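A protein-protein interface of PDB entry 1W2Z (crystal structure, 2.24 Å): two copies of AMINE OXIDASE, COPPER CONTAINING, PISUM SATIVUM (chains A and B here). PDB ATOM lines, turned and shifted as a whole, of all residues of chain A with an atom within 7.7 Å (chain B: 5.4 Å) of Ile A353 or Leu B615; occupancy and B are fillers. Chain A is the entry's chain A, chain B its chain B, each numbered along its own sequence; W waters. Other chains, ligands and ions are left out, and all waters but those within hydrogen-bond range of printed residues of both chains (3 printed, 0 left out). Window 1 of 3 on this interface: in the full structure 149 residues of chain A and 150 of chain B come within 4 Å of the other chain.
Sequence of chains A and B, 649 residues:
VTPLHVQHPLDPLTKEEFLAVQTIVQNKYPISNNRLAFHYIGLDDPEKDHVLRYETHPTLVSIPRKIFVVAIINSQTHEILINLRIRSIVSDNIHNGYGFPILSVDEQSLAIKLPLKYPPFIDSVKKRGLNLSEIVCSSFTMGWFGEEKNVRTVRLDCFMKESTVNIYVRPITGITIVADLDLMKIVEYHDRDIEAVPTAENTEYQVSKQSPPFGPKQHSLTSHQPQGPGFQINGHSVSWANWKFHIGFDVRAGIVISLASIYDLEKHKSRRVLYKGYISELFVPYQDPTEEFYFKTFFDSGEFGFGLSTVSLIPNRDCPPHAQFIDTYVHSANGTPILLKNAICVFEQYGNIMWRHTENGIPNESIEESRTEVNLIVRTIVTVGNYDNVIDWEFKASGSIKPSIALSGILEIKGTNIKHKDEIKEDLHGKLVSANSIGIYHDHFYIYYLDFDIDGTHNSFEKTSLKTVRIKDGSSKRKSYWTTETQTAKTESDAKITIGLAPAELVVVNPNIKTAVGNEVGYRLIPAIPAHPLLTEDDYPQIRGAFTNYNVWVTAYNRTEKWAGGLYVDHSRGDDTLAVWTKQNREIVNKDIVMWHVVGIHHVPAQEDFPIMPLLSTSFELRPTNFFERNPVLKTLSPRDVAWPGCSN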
ATOM      1  N   GLN A 349       8.818  19.701  13.255  1.00  0.00           N
ATOM      2  CA  GLN A 349       9.283  20.108  11.928  1.00  0.00           C
ATOM      3  C   GLN A 349      10.732  19.678  11.741  1.00  0.00           C
ATOM      4  O   GLN A 349      11.582  19.924  12.611  1.00  0.00           O
ATOM      5  CB  GLN A 349       9.171  21.610  11.797  1.00  0.00           C
ATOM      6  CG  GLN A 349       9.566  22.174  10.426  1.00  0.00           C
ATOM      7  CD  GLN A 349      10.550  23.335  10.553  1.00  0.00           C
ATOM      8  OE1 GLN A 349      10.143  24.483  10.788  1.00  0.00           O
ATOM      9  NE2 GLN A 349      11.839  23.039  10.423  1.00  0.00           N
ATOM     10  N   TYR A 350      11.012  19.038  10.609  1.00  0.00           N
ATOM     11  CA  TYR A 350      12.325  18.424  10.327  1.00  0.00           C
ATOM     12  C   TYR A 350      13.010  19.095   9.139  1.00  0.00           C
ATOM     13  O   TYR A 350      12.376  19.821   8.369  1.00  0.00           O
ATOM     14  CB  TYR A 350      12.171  16.923   9.985  1.00  0.00           C
ATOM     15  CG  TYR A 350      11.837  16.082  11.183  1.00  0.00           C
ATOM     16  CD1 TYR A 350      10.557  16.108  11.743  1.00  0.00           C
ATOM     17  CD2 TYR A 350      12.769  15.224  11.732  1.00  0.00           C
ATOM     18  CE1 TYR A 350      10.233  15.320  12.834  1.00  0.00           C
ATOM     19  CE2 TYR A 350      12.448  14.458  12.818  1.00  0.00           C
ATOM     20  CZ  TYR A 350      11.181  14.519  13.370  1.00  0.00           C
ATOM     21  OH  TYR A 350      10.872  13.760  14.469  1.00  0.00           O
ATOM     22  N   GLY A 351      14.305  18.825   9.002  1.00  0.00           N
ATOM     23  CA  GLY A 351      15.100  19.287   7.869  1.00  0.00           C
ATOM     24  C   GLY A 351      16.119  20.392   8.152  1.00  0.00           C
ATOM     25  O   GLY A 351      17.101  20.519   7.419  1.00  0.00           O
ATOM     26  N   ASN A 352      15.916  21.191   9.198  1.00  0.00           N
ATOM     27  CA  ASN A 352      16.775  22.351   9.426  1.00  0.00           C
ATOM     28  C   ASN A 352      18.150  21.880   9.893  1.00  0.00           C
ATOM     29  O   ASN A 352      18.259  20.972  10.736  1.00  0.00           O
ATOM     30  CB  ASN A 352      16.222  23.258  10.524  1.00  0.00           C
ATOM     31  CG  ASN A 352      15.040  24.113  10.092  1.00  0.00           C
ATOM     32  OD1 ASN A 352      14.280  23.774   9.210  1.00  0.00           O
ATOM     33  ND2 ASN A 352      14.879  25.239  10.770  1.00  0.00           N
ATOM     34  N   ILE A 353      19.189  22.531   9.378  1.00  0.00           N
ATOM     35  CA  ILE A 353      20.527  22.388   9.909  1.00  0.00           C
ATOM     36  C   ILE A 353      20.591  23.112  11.266  1.00  0.00           C
ATOM     37  O   ILE A 353      20.169  24.251  11.384  1.00  0.00           O
ATOM     38  CB  ILE A 353      21.551  22.980   8.909  1.00  0.00           C
ATOM     39  CG1 ILE A 353      21.460  22.244   7.566  1.00  0.00           C
ATOM     40  CG2 ILE A 353      22.982  22.915   9.481  1.00  0.00           C
ATOM     41  CD1 ILE A 353      22.173  22.935   6.443  1.00  0.00           C
ATOM     42  N   MET A 354      21.118  22.439  12.277  1.00  0.00           N
ATOM     43  CA  MET A 354      21.234  22.986  13.620  1.00  0.00           C
ATOM     44  C   MET A 354      22.519  23.796  13.720  1.00  0.00           C
ATOM     45  O   MET A 354      22.529  24.924  14.216  1.00  0.00           O
ATOM     46  CB  MET A 354      21.244  21.828  14.609  1.00  0.00           C
ATOM     47  CG  MET A 354      21.163  22.238  16.046  1.00  0.00           C
ATOM     48  SD  MET A 354      20.678  20.840  17.088  1.00  0.00           S
ATOM     49  CE  MET A 354      21.951  19.641  16.722  1.00  0.00           C
ATOM     50  N   TRP A 355      23.596  23.196  13.230  1.00  0.00           N
ATOM     51  CA  TRP A 355      24.851  23.872  13.081  1.00  0.00           C
ATOM     52  C   TRP A 355      25.800  22.963  12.346  1.00  0.00           C
ATOM     53  O   TRP A 355      25.534  21.780  12.211  1.00  0.00           O
ATOM     54  CB  TRP A 355      25.451  24.283  14.431  1.00  0.00           C
ATOM     55  CG  TRP A 355      25.497  23.238  15.533  1.00  0.00           C
ATOM     56  CD1 TRP A 355      24.676  23.167  16.620  1.00  0.00           C
ATOM     57  CD2 TRP A 355      26.495  22.217  15.717  1.00  0.00           C
ATOM     58  NE1 TRP A 355      25.060  22.125  17.437  1.00  0.00           N
ATOM     59  CE2 TRP A 355      26.175  21.526  16.914  1.00  0.00           C
ATOM     60  CE3 TRP A 355      27.621  21.804  14.984  1.00  0.00           C
ATOM     61  CZ2 TRP A 355      26.942  20.455  17.394  1.00  0.00           C
ATOM     62  CZ3 TRP A 355      28.374  20.727  15.455  1.00  0.00           C
ATOM     63  CH2 TRP A 355      28.035  20.071  16.652  1.00  0.00           C
ATOM     64  N   ARG A 356      26.913  23.521  11.887  1.00  0.00           N
ATOM     65  CA  ARG A 356      27.886  22.748  11.120  1.00  0.00           C
ATOM     66  C   ARG A 356      29.238  23.428  11.032  1.00  0.00           C
ATOM     67  O   ARG A 356      29.356  24.645  11.230  1.00  0.00           O
ATOM     68  CB  ARG A 356      27.361  22.498   9.695  1.00  0.00           C
ATOM     69  CG  ARG A 356      27.596  23.627   8.752  1.00  0.00           C
ATOM     70  CD  ARG A 356      27.119  23.388   7.336  1.00  0.00           C
ATOM     71  NE  ARG A 356      27.496  22.087   6.803  1.00  0.00           N
ATOM     72  CZ  ARG A 356      28.713  21.751   6.384  1.00  0.00           C
ATOM     73  NH1 ARG A 356      29.725  22.590   6.450  1.00  0.00           N
ATOM     74  NH2 ARG A 356      28.916  20.539   5.911  1.00  0.00           N
ATOM     75  N   HIS A 357      30.259  22.628  10.725  1.00  0.00           N
ATOM     76  CA  HIS A 357      31.531  23.147  10.226  1.00  0.00           C
ATOM     77  C   HIS A 357      32.269  22.097   9.417  1.00  0.00           C
ATOM     78  O   HIS A 357      32.346  20.946   9.812  1.00  0.00           O
ATOM     79  CB  HIS A 357      32.451  23.634  11.356  1.00  0.00           C
ATOM     80  CG  HIS A 357      33.688  24.332  10.866  1.00  0.00           C
ATOM     81  ND1 HIS A 357      33.646  25.393   9.990  1.00  0.00           N
ATOM     82  CD2 HIS A 357      34.999  24.107  11.114  1.00  0.00           C
ATOM     83  CE1 HIS A 357      34.874  25.810   9.742  1.00  0.00           C
ATOM     84  NE2 HIS A 357      35.715  25.047  10.410  1.00  0.00           N
ATOM     85  N   GLU A 369      31.420  18.184  10.271  1.00  0.00           N
ATOM     86  CA  GLU A 369      30.328  17.840  11.180  1.00  0.00           C
ATOM     87  C   GLU A 369      29.150  18.717  10.811  1.00  0.00           C
ATOM     88  O   GLU A 369      29.275  19.946  10.735  1.00  0.00           O
ATOM     89  CB  GLU A 369      30.729  18.116  12.636  1.00  0.00           C
ATOM     90  CG  GLU A 369      29.677  17.723  13.679  1.00  0.00           C
ATOM     91  CD  GLU A 369      29.714  16.249  14.039  1.00  0.00           C
ATOM     92  OE1 GLU A 369      30.663  15.524  13.628  1.00  0.00           O
ATOM     93  OE2 GLU A 369      28.803  15.813  14.758  1.00  0.00           O
ATOM     94  N   SER A 370      28.023  18.085  10.545  1.00  0.00           N
ATOM     95  CA  SER A 370      26.769  18.795  10.331  1.00  0.00           C
ATOM     96  C   SER A 370      25.660  18.040  11.050  1.00  0.00           C
ATOM     97  O   SER A 370      25.500  16.834  10.847  1.00  0.00           O
ATOM     98  CB  SER A 370      26.454  18.922   8.842  1.00  0.00           C
ATOM     99  OG  SER A 370      25.178  19.520   8.684  1.00  0.00           O
ATOM    100  N   ARG A 371      24.926  18.752  11.901  1.00  0.00           N
ATOM    101  CA  ARG A 371      23.830  18.185  12.665  1.00  0.00           C
ATOM    102  C   ARG A 371      22.536  18.881  12.350  1.00  0.00           C
ATOM    103  O   ARG A 371      22.533  20.059  11.998  1.00  0.00           O
ATOM    104  CB  ARG A 371      24.117  18.294  14.150  1.00  0.00           C
ATOM    105  CG  ARG A 371      25.269  17.476  14.554  1.00  0.00           C
ATOM    106  CD  ARG A 371      25.403  17.372  16.031  1.00  0.00           C
ATOM    107  NE  ARG A 371      26.750  17.024  16.443  1.00  0.00           N
ATOM    108  CZ  ARG A 371      27.153  16.962  17.696  1.00  0.00           C
ATOM    109  NH1 ARG A 371      26.318  17.195  18.701  1.00  0.00           N
ATOM    110  NH2 ARG A 371      28.411  16.653  17.951  1.00  0.00           N
ATOM    111  N   THR A 372      21.435  18.138  12.468  1.00  0.00           N
ATOM    112  CA  THR A 372      20.116  18.681  12.234  1.00  0.00           C
ATOM    113  C   THR A 372      19.318  18.789  13.521  1.00  0.00           C
ATOM    114  O   THR A 372      19.544  18.061  14.499  1.00  0.00           O
ATOM    115  CB  THR A 372      19.282  17.829  11.241  1.00  0.00           C
ATOM    116  OG1 THR A 372      19.193  16.474  11.698  1.00  0.00           O
ATOM    117  CG2 THR A 372      19.896  17.762   9.848  1.00  0.00           C
ATOM    118  N   GLU A 373      18.341  19.685  13.486  1.00  0.00           N
ATOM    119  CA  GLU A 373      17.451  19.928  14.619  1.00  0.00           C
ATOM    120  C   GLU A 373      16.034  19.522  14.270  1.00  0.00           C
ATOM    121  O   GLU A 373      15.623  19.550  13.108  1.00  0.00           O
ATOM    122  CB  GLU A 373      17.466  21.414  14.998  1.00  0.00           C
ATOM    123  CG  GLU A 373      17.112  22.387  13.874  1.00  0.00           C
ATOM    124  CD  GLU A 373      17.270  23.856  14.267  1.00  0.00           C
ATOM    125  OE1 GLU A 373      18.110  24.173  15.144  1.00  0.00           O
ATOM    126  OE2 GLU A 373      16.535  24.694  13.697  1.00  0.00           O
ATOM    127  N   ASN A 375      12.357  20.881  15.352  1.00  0.00           N
ATOM    128  CA  ASN A 375      11.702  22.024  15.962  1.00  0.00           C
ATOM    129  C   ASN A 375      10.229  21.728  16.280  1.00  0.00           C
ATOM    130  O   ASN A 375       9.627  20.834  15.708  1.00  0.00           O
ATOM    131  CB  ASN A 375      11.826  23.231  15.040  1.00  0.00           C
ATOM    132  CG  ASN A 375      13.265  23.602  14.755  1.00  0.00           C
ATOM    133  OD1 ASN A 375      14.130  23.577  15.651  1.00  0.00           O
ATOM    134  ND2 ASN A 375      13.540  23.959  13.513  1.00  0.00           N
ATOM    135  N   LYS A 396      12.859  25.858  19.666  1.00  0.00           N
ATOM    136  CA  LYS A 396      14.033  25.129  19.206  1.00  0.00           C
ATOM    137  C   LYS A 396      14.876  24.701  20.387  1.00  0.00           C
ATOM    138  O   LYS A 396      14.947  25.420  21.381  1.00  0.00           O
ATOM    139  CB  LYS A 396      14.859  26.013  18.277  1.00  0.00           C
ATOM    140  CG  LYS A 396      14.037  26.483  17.092  1.00  0.00           C
ATOM    141  CD  LYS A 396      14.758  27.517  16.241  1.00  0.00           C
ATOM    142  CE  LYS A 396      15.692  26.897  15.292  1.00  0.00           C
ATOM    143  NZ  LYS A 396      17.042  27.472  15.416  1.00  0.00           N
ATOM    144  N   SER A 398      17.920  24.823  20.595  1.00  0.00           N
ATOM    145  CA  SER A 398      18.952  25.852  20.735  1.00  0.00           C
ATOM    146  C   SER A 398      18.501  27.002  21.648  1.00  0.00           C
ATOM    147  O   SER A 398      19.306  27.858  22.020  1.00  0.00           O
ATOM    148  CB  SER A 398      19.352  26.435  19.381  1.00  0.00           C
ATOM    149  OG  SER A 398      18.279  27.173  18.801  1.00  0.00           O
ATOM    150  N   SER A 400      16.046  29.262  20.957  1.00  0.00           N
ATOM    151  CA  SER A 400      15.302  30.273  20.226  1.00  0.00           C
ATOM    152  C   SER A 400      13.812  29.972  20.269  1.00  0.00           C
ATOM    153  O   SER A 400      13.399  28.806  20.218  1.00  0.00           O
ATOM    154  CB  SER A 400      15.762  30.318  18.760  1.00  0.00           C
ATOM    155  OG  SER A 400      17.021  30.947  18.647  1.00  0.00           O
ATOM    156  N   GLU A 621      12.538  36.515  16.014  1.00  0.00           N
ATOM    157  CA  GLU A 621      13.222  35.504  16.796  1.00  0.00           C
ATOM    158  C   GLU A 621      13.579  36.095  18.153  1.00  0.00           C
ATOM    159  O   GLU A 621      14.011  37.236  18.246  1.00  0.00           O
ATOM    160  CB  GLU A 621      14.495  35.050  16.063  1.00  0.00           C
ATOM    161  CG  GLU A 621      15.286  33.949  16.771  1.00  0.00           C
ATOM    162  CD  GLU A 621      16.508  33.449  16.010  1.00  0.00           C
ATOM    163  OE1 GLU A 621      16.801  33.945  14.875  1.00  0.00           O
ATOM    164  OE2 GLU A 621      17.182  32.548  16.580  1.00  0.00           O
ATOM    165  N   ARG A 623      16.252  35.147  20.771  1.00  0.00           N
ATOM    166  CA  ARG A 623      17.468  34.319  20.683  1.00  0.00           C
ATOM    167  C   ARG A 623      18.280  34.413  21.974  1.00  0.00           C
ATOM    168  O   ARG A 623      18.604  35.511  22.387  1.00  0.00           O
ATOM    169  CB  ARG A 623      18.330  34.805  19.523  1.00  0.00           C
ATOM    170  CG  ARG A 623      19.435  33.862  19.087  1.00  0.00           C
ATOM    171  CD  ARG A 623      19.970  34.170  17.659  1.00  0.00           C
ATOM    172  NE  ARG A 623      21.102  33.310  17.289  1.00  0.00           N
ATOM    173  CZ  ARG A 623      21.075  32.335  16.385  1.00  0.00           C
ATOM    174  NH1 ARG A 623      19.960  32.029  15.726  1.00  0.00           N
ATOM    175  NH2 ARG A 623      22.170  31.648  16.145  1.00  0.00           N
ATOM    176  N   ASN A 631      27.155  27.166  23.509  1.00  0.00           N
ATOM    177  CA  ASN A 631      26.153  26.597  22.580  1.00  0.00           C
ATOM    178  C   ASN A 631      25.344  25.480  23.277  1.00  0.00           C
ATOM    179  O   ASN A 631      25.891  24.448  23.595  1.00  0.00           O
ATOM    180  CB  ASN A 631      26.873  26.062  21.336  1.00  0.00           C
ATOM    181  CG  ASN A 631      25.928  25.385  20.321  1.00  0.00           C
ATOM    182  OD1 ASN A 631      24.803  25.099  20.638  1.00  0.00           O
ATOM    183  ND2 ASN A 631      26.425  25.108  19.095  1.00  0.00           N
ATOM    184  N   VAL A 633      23.200  23.435  22.240  1.00  0.00           N
ATOM    185  CA  VAL A 633      23.031  22.218  21.444  1.00  0.00           C
ATOM    186  C   VAL A 633      24.382  21.632  20.962  1.00  0.00           C
ATOM    187  O   VAL A 633      24.439  20.826  19.997  1.00  0.00           O
ATOM    188  CB  VAL A 633      21.976  22.424  20.288  1.00  0.00           C
ATOM    189  CG1 VAL A 633      20.585  22.606  20.873  1.00  0.00           C
ATOM    190  CG2 VAL A 633      22.322  23.632  19.383  1.00  0.00           C
ATOM    191  N   ARG B 317      21.972  15.293   6.344  1.00  0.00           N
ATOM    192  CA  ARG B 317      22.273  16.329   7.325  1.00  0.00           C
ATOM    193  C   ARG B 317      22.221  17.722   6.683  1.00  0.00           C
ATOM    194  O   ARG B 317      21.417  18.537   7.060  1.00  0.00           O
ATOM    195  CB  ARG B 317      23.637  16.050   7.972  1.00  0.00           C
ATOM    196  CG  ARG B 317      23.728  14.624   8.630  1.00  0.00           C
ATOM    197  CD  ARG B 317      22.868  14.427   9.891  1.00  0.00           C
ATOM    198  NE  ARG B 317      23.294  13.244  10.652  1.00  0.00           N
ATOM    199  CZ  ARG B 317      24.272  13.202  11.595  1.00  0.00           C
ATOM    200  NH1 ARG B 317      24.952  14.289  11.959  1.00  0.00           N
ATOM    201  NH2 ARG B 317      24.543  12.045  12.215  1.00  0.00           N
ATOM    202  N   ASP B 318      23.102  17.993   5.731  1.00  0.00           N
ATOM    203  CA  ASP B 318      23.106  19.259   5.015  1.00  0.00           C
ATOM    204  C   ASP B 318      21.897  19.410   4.107  1.00  0.00           C
ATOM    205  O   ASP B 318      21.485  20.524   3.816  1.00  0.00           O
ATOM    206  CB  ASP B 318      24.385  19.394   4.170  1.00  0.00           C
ATOM    207  CG  ASP B 318      25.615  19.627   5.008  1.00  0.00           C
ATOM    208  OD1 ASP B 318      25.472  20.223   6.076  1.00  0.00           O
ATOM    209  OD2 ASP B 318      26.771  19.274   4.674  1.00  0.00           O
ATOM    210  N   ARG B 379      20.413  23.973  -2.763  1.00  0.00           N
ATOM    211  CA  ARG B 379      21.295  24.344  -1.699  1.00  0.00           C
ATOM    212  C   ARG B 379      22.751  24.030  -2.020  1.00  0.00           C
ATOM    213  O   ARG B 379      23.076  23.034  -2.647  1.00  0.00           O
ATOM    214  CB  ARG B 379      20.852  23.630  -0.439  1.00  0.00           C
ATOM    215  CG  ARG B 379      21.823  23.619   0.713  1.00  0.00           C
ATOM    216  CD  ARG B 379      21.207  23.004   1.974  1.00  0.00           C
ATOM    217  NE  ARG B 379      20.144  23.855   2.485  1.00  0.00           N
ATOM    218  CZ  ARG B 379      19.178  23.474   3.318  1.00  0.00           C
ATOM    219  NH1 ARG B 379      19.119  22.235   3.760  1.00  0.00           N
ATOM    220  NH2 ARG B 379      18.254  24.357   3.705  1.00  0.00           N
ATOM    221  N   ILE B 381      26.855  24.834   0.030  1.00  0.00           N
ATOM    222  CA  ILE B 381      27.495  25.306   1.261  1.00  0.00           C
ATOM    223  C   ILE B 381      28.936  25.685   0.979  1.00  0.00           C
ATOM    224  O   ILE B 381      29.692  24.917   0.394  1.00  0.00           O
ATOM    225  CB  ILE B 381      27.406  24.285   2.406  1.00  0.00           C
ATOM    226  CG1 ILE B 381      25.934  24.087   2.809  1.00  0.00           C
ATOM    227  CG2 ILE B 381      28.266  24.749   3.616  1.00  0.00           C
ATOM    228  CD1 ILE B 381      25.718  23.133   3.973  1.00  0.00           C
ATOM    229  N   VAL B 390      25.414  28.589   4.357  1.00  0.00           N
ATOM    230  CA  VAL B 390      24.443  27.759   3.695  1.00  0.00           C
ATOM    231  C   VAL B 390      23.614  28.656   2.755  1.00  0.00           C
ATOM    232  O   VAL B 390      22.832  29.498   3.203  1.00  0.00           O
ATOM    233  CB  VAL B 390      23.557  27.051   4.724  1.00  0.00           C
ATOM    234  CG1 VAL B 390      22.630  26.066   4.063  1.00  0.00           C
ATOM    235  CG2 VAL B 390      24.442  26.334   5.795  1.00  0.00           C
ATOM    236  N   ALA B 406      22.305  31.167   5.473  1.00  0.00           N
ATOM    237  CA  ALA B 406      22.400  30.854   6.893  1.00  0.00           C
ATOM    238  C   ALA B 406      23.867  30.694   7.245  1.00  0.00           C
ATOM    239  O   ALA B 406      24.639  30.190   6.442  1.00  0.00           O
ATOM    240  CB  ALA B 406      21.621  29.601   7.210  1.00  0.00           C
ATOM    241  N   LEU B 407      24.234  31.125   8.446  1.00  0.00           N
ATOM    242  CA  LEU B 407      25.606  31.172   8.903  1.00  0.00           C
ATOM    243  C   LEU B 407      25.799  30.199  10.068  1.00  0.00           C
ATOM    244  O   LEU B 407      24.970  30.134  10.955  1.00  0.00           O
ATOM    245  CB  LEU B 407      25.906  32.585   9.431  1.00  0.00           C
ATOM    246  CG  LEU B 407      27.104  33.335   8.885  1.00  0.00           C
ATOM    247  CD1 LEU B 407      27.018  34.813   9.289  1.00  0.00           C
ATOM    248  CD2 LEU B 407      28.397  32.684   9.372  1.00  0.00           C
ATOM    249  N   SER B 408      26.890  29.444  10.032  1.00  0.00           N
ATOM    250  CA  SER B 408      27.364  28.656  11.147  1.00  0.00           C
ATOM    251  C   SER B 408      28.900  28.623  11.103  1.00  0.00           C
ATOM    252  O   SER B 408      29.512  29.509  10.490  1.00  0.00           O
ATOM    253  CB  SER B 408      26.811  27.237  11.090  1.00  0.00           C
ATOM    254  OG  SER B 408      27.057  26.552  12.312  1.00  0.00           O
ATOM    255  N   MET B 613      28.742  27.594  16.368  1.00  0.00           N
ATOM    256  CA  MET B 613      27.577  28.449  16.451  1.00  0.00           C
ATOM    257  C   MET B 613      26.308  27.900  15.789  1.00  0.00           C
ATOM    258  O   MET B 613      26.331  27.441  14.637  1.00  0.00           O
ATOM    259  CB  MET B 613      27.905  29.853  15.959  1.00  0.00           C
ATOM    260  CG  MET B 613      27.958  30.094  14.493  1.00  0.00           C
ATOM    261  SD  MET B 613      28.376  31.848  14.185  1.00  0.00           S
ATOM    262  CE  MET B 613      30.142  31.751  14.338  1.00  0.00           C
ATOM    263  N   PRO B 614      25.204  27.953  16.536  1.00  0.00           N
ATOM    264  CA  PRO B 614      23.896  27.598  15.978  1.00  0.00           C
ATOM    265  C   PRO B 614      23.550  28.487  14.796  1.00  0.00           C
ATOM    266  O   PRO B 614      23.875  29.685  14.809  1.00  0.00           O
ATOM    267  CB  PRO B 614      22.919  27.862  17.133  1.00  0.00           C
ATOM    268  CG  PRO B 614      23.758  27.906  18.375  1.00  0.00           C
ATOM    269  CD  PRO B 614      25.118  28.351  17.949  1.00  0.00           C
ATOM    270  N   LEU B 615      22.841  27.912  13.834  1.00  0.00           N
ATOM    271  CA  LEU B 615      22.503  28.572  12.583  1.00  0.00           C
ATOM    272  C   LEU B 615      21.805  29.900  12.812  1.00  0.00           C
ATOM    273  O   LEU B 615      20.847  29.980  13.611  1.00  0.00           O
ATOM    274  CB  LEU B 615      21.573  27.681  11.765  1.00  0.00           C
ATOM    275  CG  LEU B 615      21.665  27.755  10.243  1.00  0.00           C
ATOM    276  CD1 LEU B 615      23.013  27.262   9.804  1.00  0.00           C
ATOM    277  CD2 LEU B 615      20.569  26.939   9.569  1.00  0.00           C
ATOM    278  N   LEU B 616      22.300  30.945  12.151  1.00  0.00           N
ATOM    279  CA  LEU B 616      21.571  32.210  12.076  1.00  0.00           C
ATOM    280  C   LEU B 616      21.091  32.356  10.643  1.00  0.00           C
ATOM    281  O   LEU B 616      21.911  32.464   9.751  1.00  0.00           O
ATOM    282  CB  LEU B 616      22.485  33.367  12.476  1.00  0.00           C
ATOM    283  CG  LEU B 616      21.873  34.778  12.387  1.00  0.00           C
ATOM    284  CD1 LEU B 616      20.827  35.045  13.471  1.00  0.00           C
ATOM    285  CD2 LEU B 616      22.951  35.838  12.436  1.00  0.00           C
ATOM    286  N   SER B 617      19.773  32.334  10.434  1.00  0.00           N
ATOM    287  CA  SER B 617      19.178  32.342   9.091  1.00  0.00           C
ATOM    288  C   SER B 617      18.673  33.725   8.654  1.00  0.00           C
ATOM    289  O   SER B 617      17.956  34.421   9.388  1.00  0.00           O
ATOM    290  CB  SER B 617      18.007  31.383   9.015  1.00  0.00           C
ATOM    291  OG  SER B 617      18.380  30.107   9.436  1.00  0.00           O
HETATM  292  O   HOH W   1      18.621  18.683   6.280  1.00  0.00           O
HETATM  293  O   HOH W   2      19.717  28.479  15.389  1.00  0.00           O
HETATM  294  O   HOH W   3      18.169  32.626  12.999  1.00  0.00           O
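The backbone NH of Arg A356 lies within hydrogen-bond range of the side-chain hydroxyl of Ser B408, 3.1 Å away. The side-chain hydroxyl (OG) of Ser A370 is in hydrogen-bond range of the side-chain carboxylate (OD1) of Asp B318 (2.7 Å). O of Met A354 lies within hydrogen-bond range of N of Leu B615, at 3.0 Å. The backbone carbonyl oxygen (O) of Leu B615 lies within hydrogen-bond range of the guanidinium group (NH1) of Arg A623 (3.1 Å). The backbone carbonyl oxygen (O) of Ser A370 sits at hydrogen-bond distance from the guanidinium group (NH1) of Arg B317, at 2.8 Å. The side-chain carboxylate of Asp B318 lies within salt-bridge range of the guanidinium group of Arg A356 (2.8 Å). The guanidinium group (NH2) of Arg A623 lies within hydrogen-bond range of the backbone carbonyl oxygen (O) of Pro B614 (2.9 Å).
Ile A353 touches four residues of chain B. Of the printed residues of chain B, Trp A355 touches Ser B408, Met B613 and Pro B614. Of the printed residues of chain B, Asn A631 touches Pro B614. Asn A375 touches none of the printed residues of chain B. Ser B617 touches none of the printed residues of chain A.
Of the 13 printed residues of chain B, 9 touch a printed residue of chain A. Of the 22 printed residues of chain A, 8 touch a printed residue of chain B. Printed residues of chain A that touch a printed residue of chain B: Ile A353, Met A354, Trp A355, Arg A356, Ser A370, Thr A372, Arg A623 and Asn A631. Hydrophobic or aromatic side chains of chain A that line the printed part of chain B: Ile A353 and Trp A355. Among the printed residues, 19 pairs touch across the chains. Among the printed residues, Asp or Glu carboxylates within 4 Å of a Lys or Arg side-chain nitrogen of the other chain: Arg A356 with Asp B318.
Water W2 bridges O of Leu B615 (2.6 Å) and NZ of Lys A396 (2.9 Å). Water W1 bridges the backbone carbonyl oxygen (O) of Gly A351 (2.6 Å) and the backbone carbonyl oxygen (O) of Arg B317 (2.9 Å). Water W3 lies within hydrogen-bond range of OE1 of Glu A621, N of Ser B617 and NH1 of Arg A623.
N of Met A354 is in hydrogen-bond range of O of Arg A371 (2.8 Å). N of Arg A371 lies within hydrogen-bond range of O of Trp A355, at 3.1 Å. The backbone carbonyl oxygen (O) of Leu B616 is in hydrogen-bond range of the backbone NH (N) of Leu B407 (3.0 Å). The side-chain amide oxygen of Asn A631 is in hydrogen-bond range of the backbone NH of Val A633 (2.8 Å). OE2 of Glu A621 lies within salt-bridge range of NH1 of Arg A623 (3.0 Å).
No position is printed for both chains.
Ile A353 touches Asp B318. Ile A353 touches Val B390. Ile A353 touches Leu B615 (O to CD2, 3.3 Å). Met A354 touches Pro B614 (O to CA, 3.5 Å). CB of Trp A355 touches OG of Ser B408 (3.5 Å). O of Met B613 touches CB of Trp A355, 3.3 Å away. Pro B614 touches Trp A355. Arg A356 touches Ile B381 (NE to CD1, 3.5 Å). Arg A623 touches Leu B616 (NH1 to CD1, 3.9 Å). CD of Pro B614 touches ND2 of Asn A631, 3.7 Å away.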
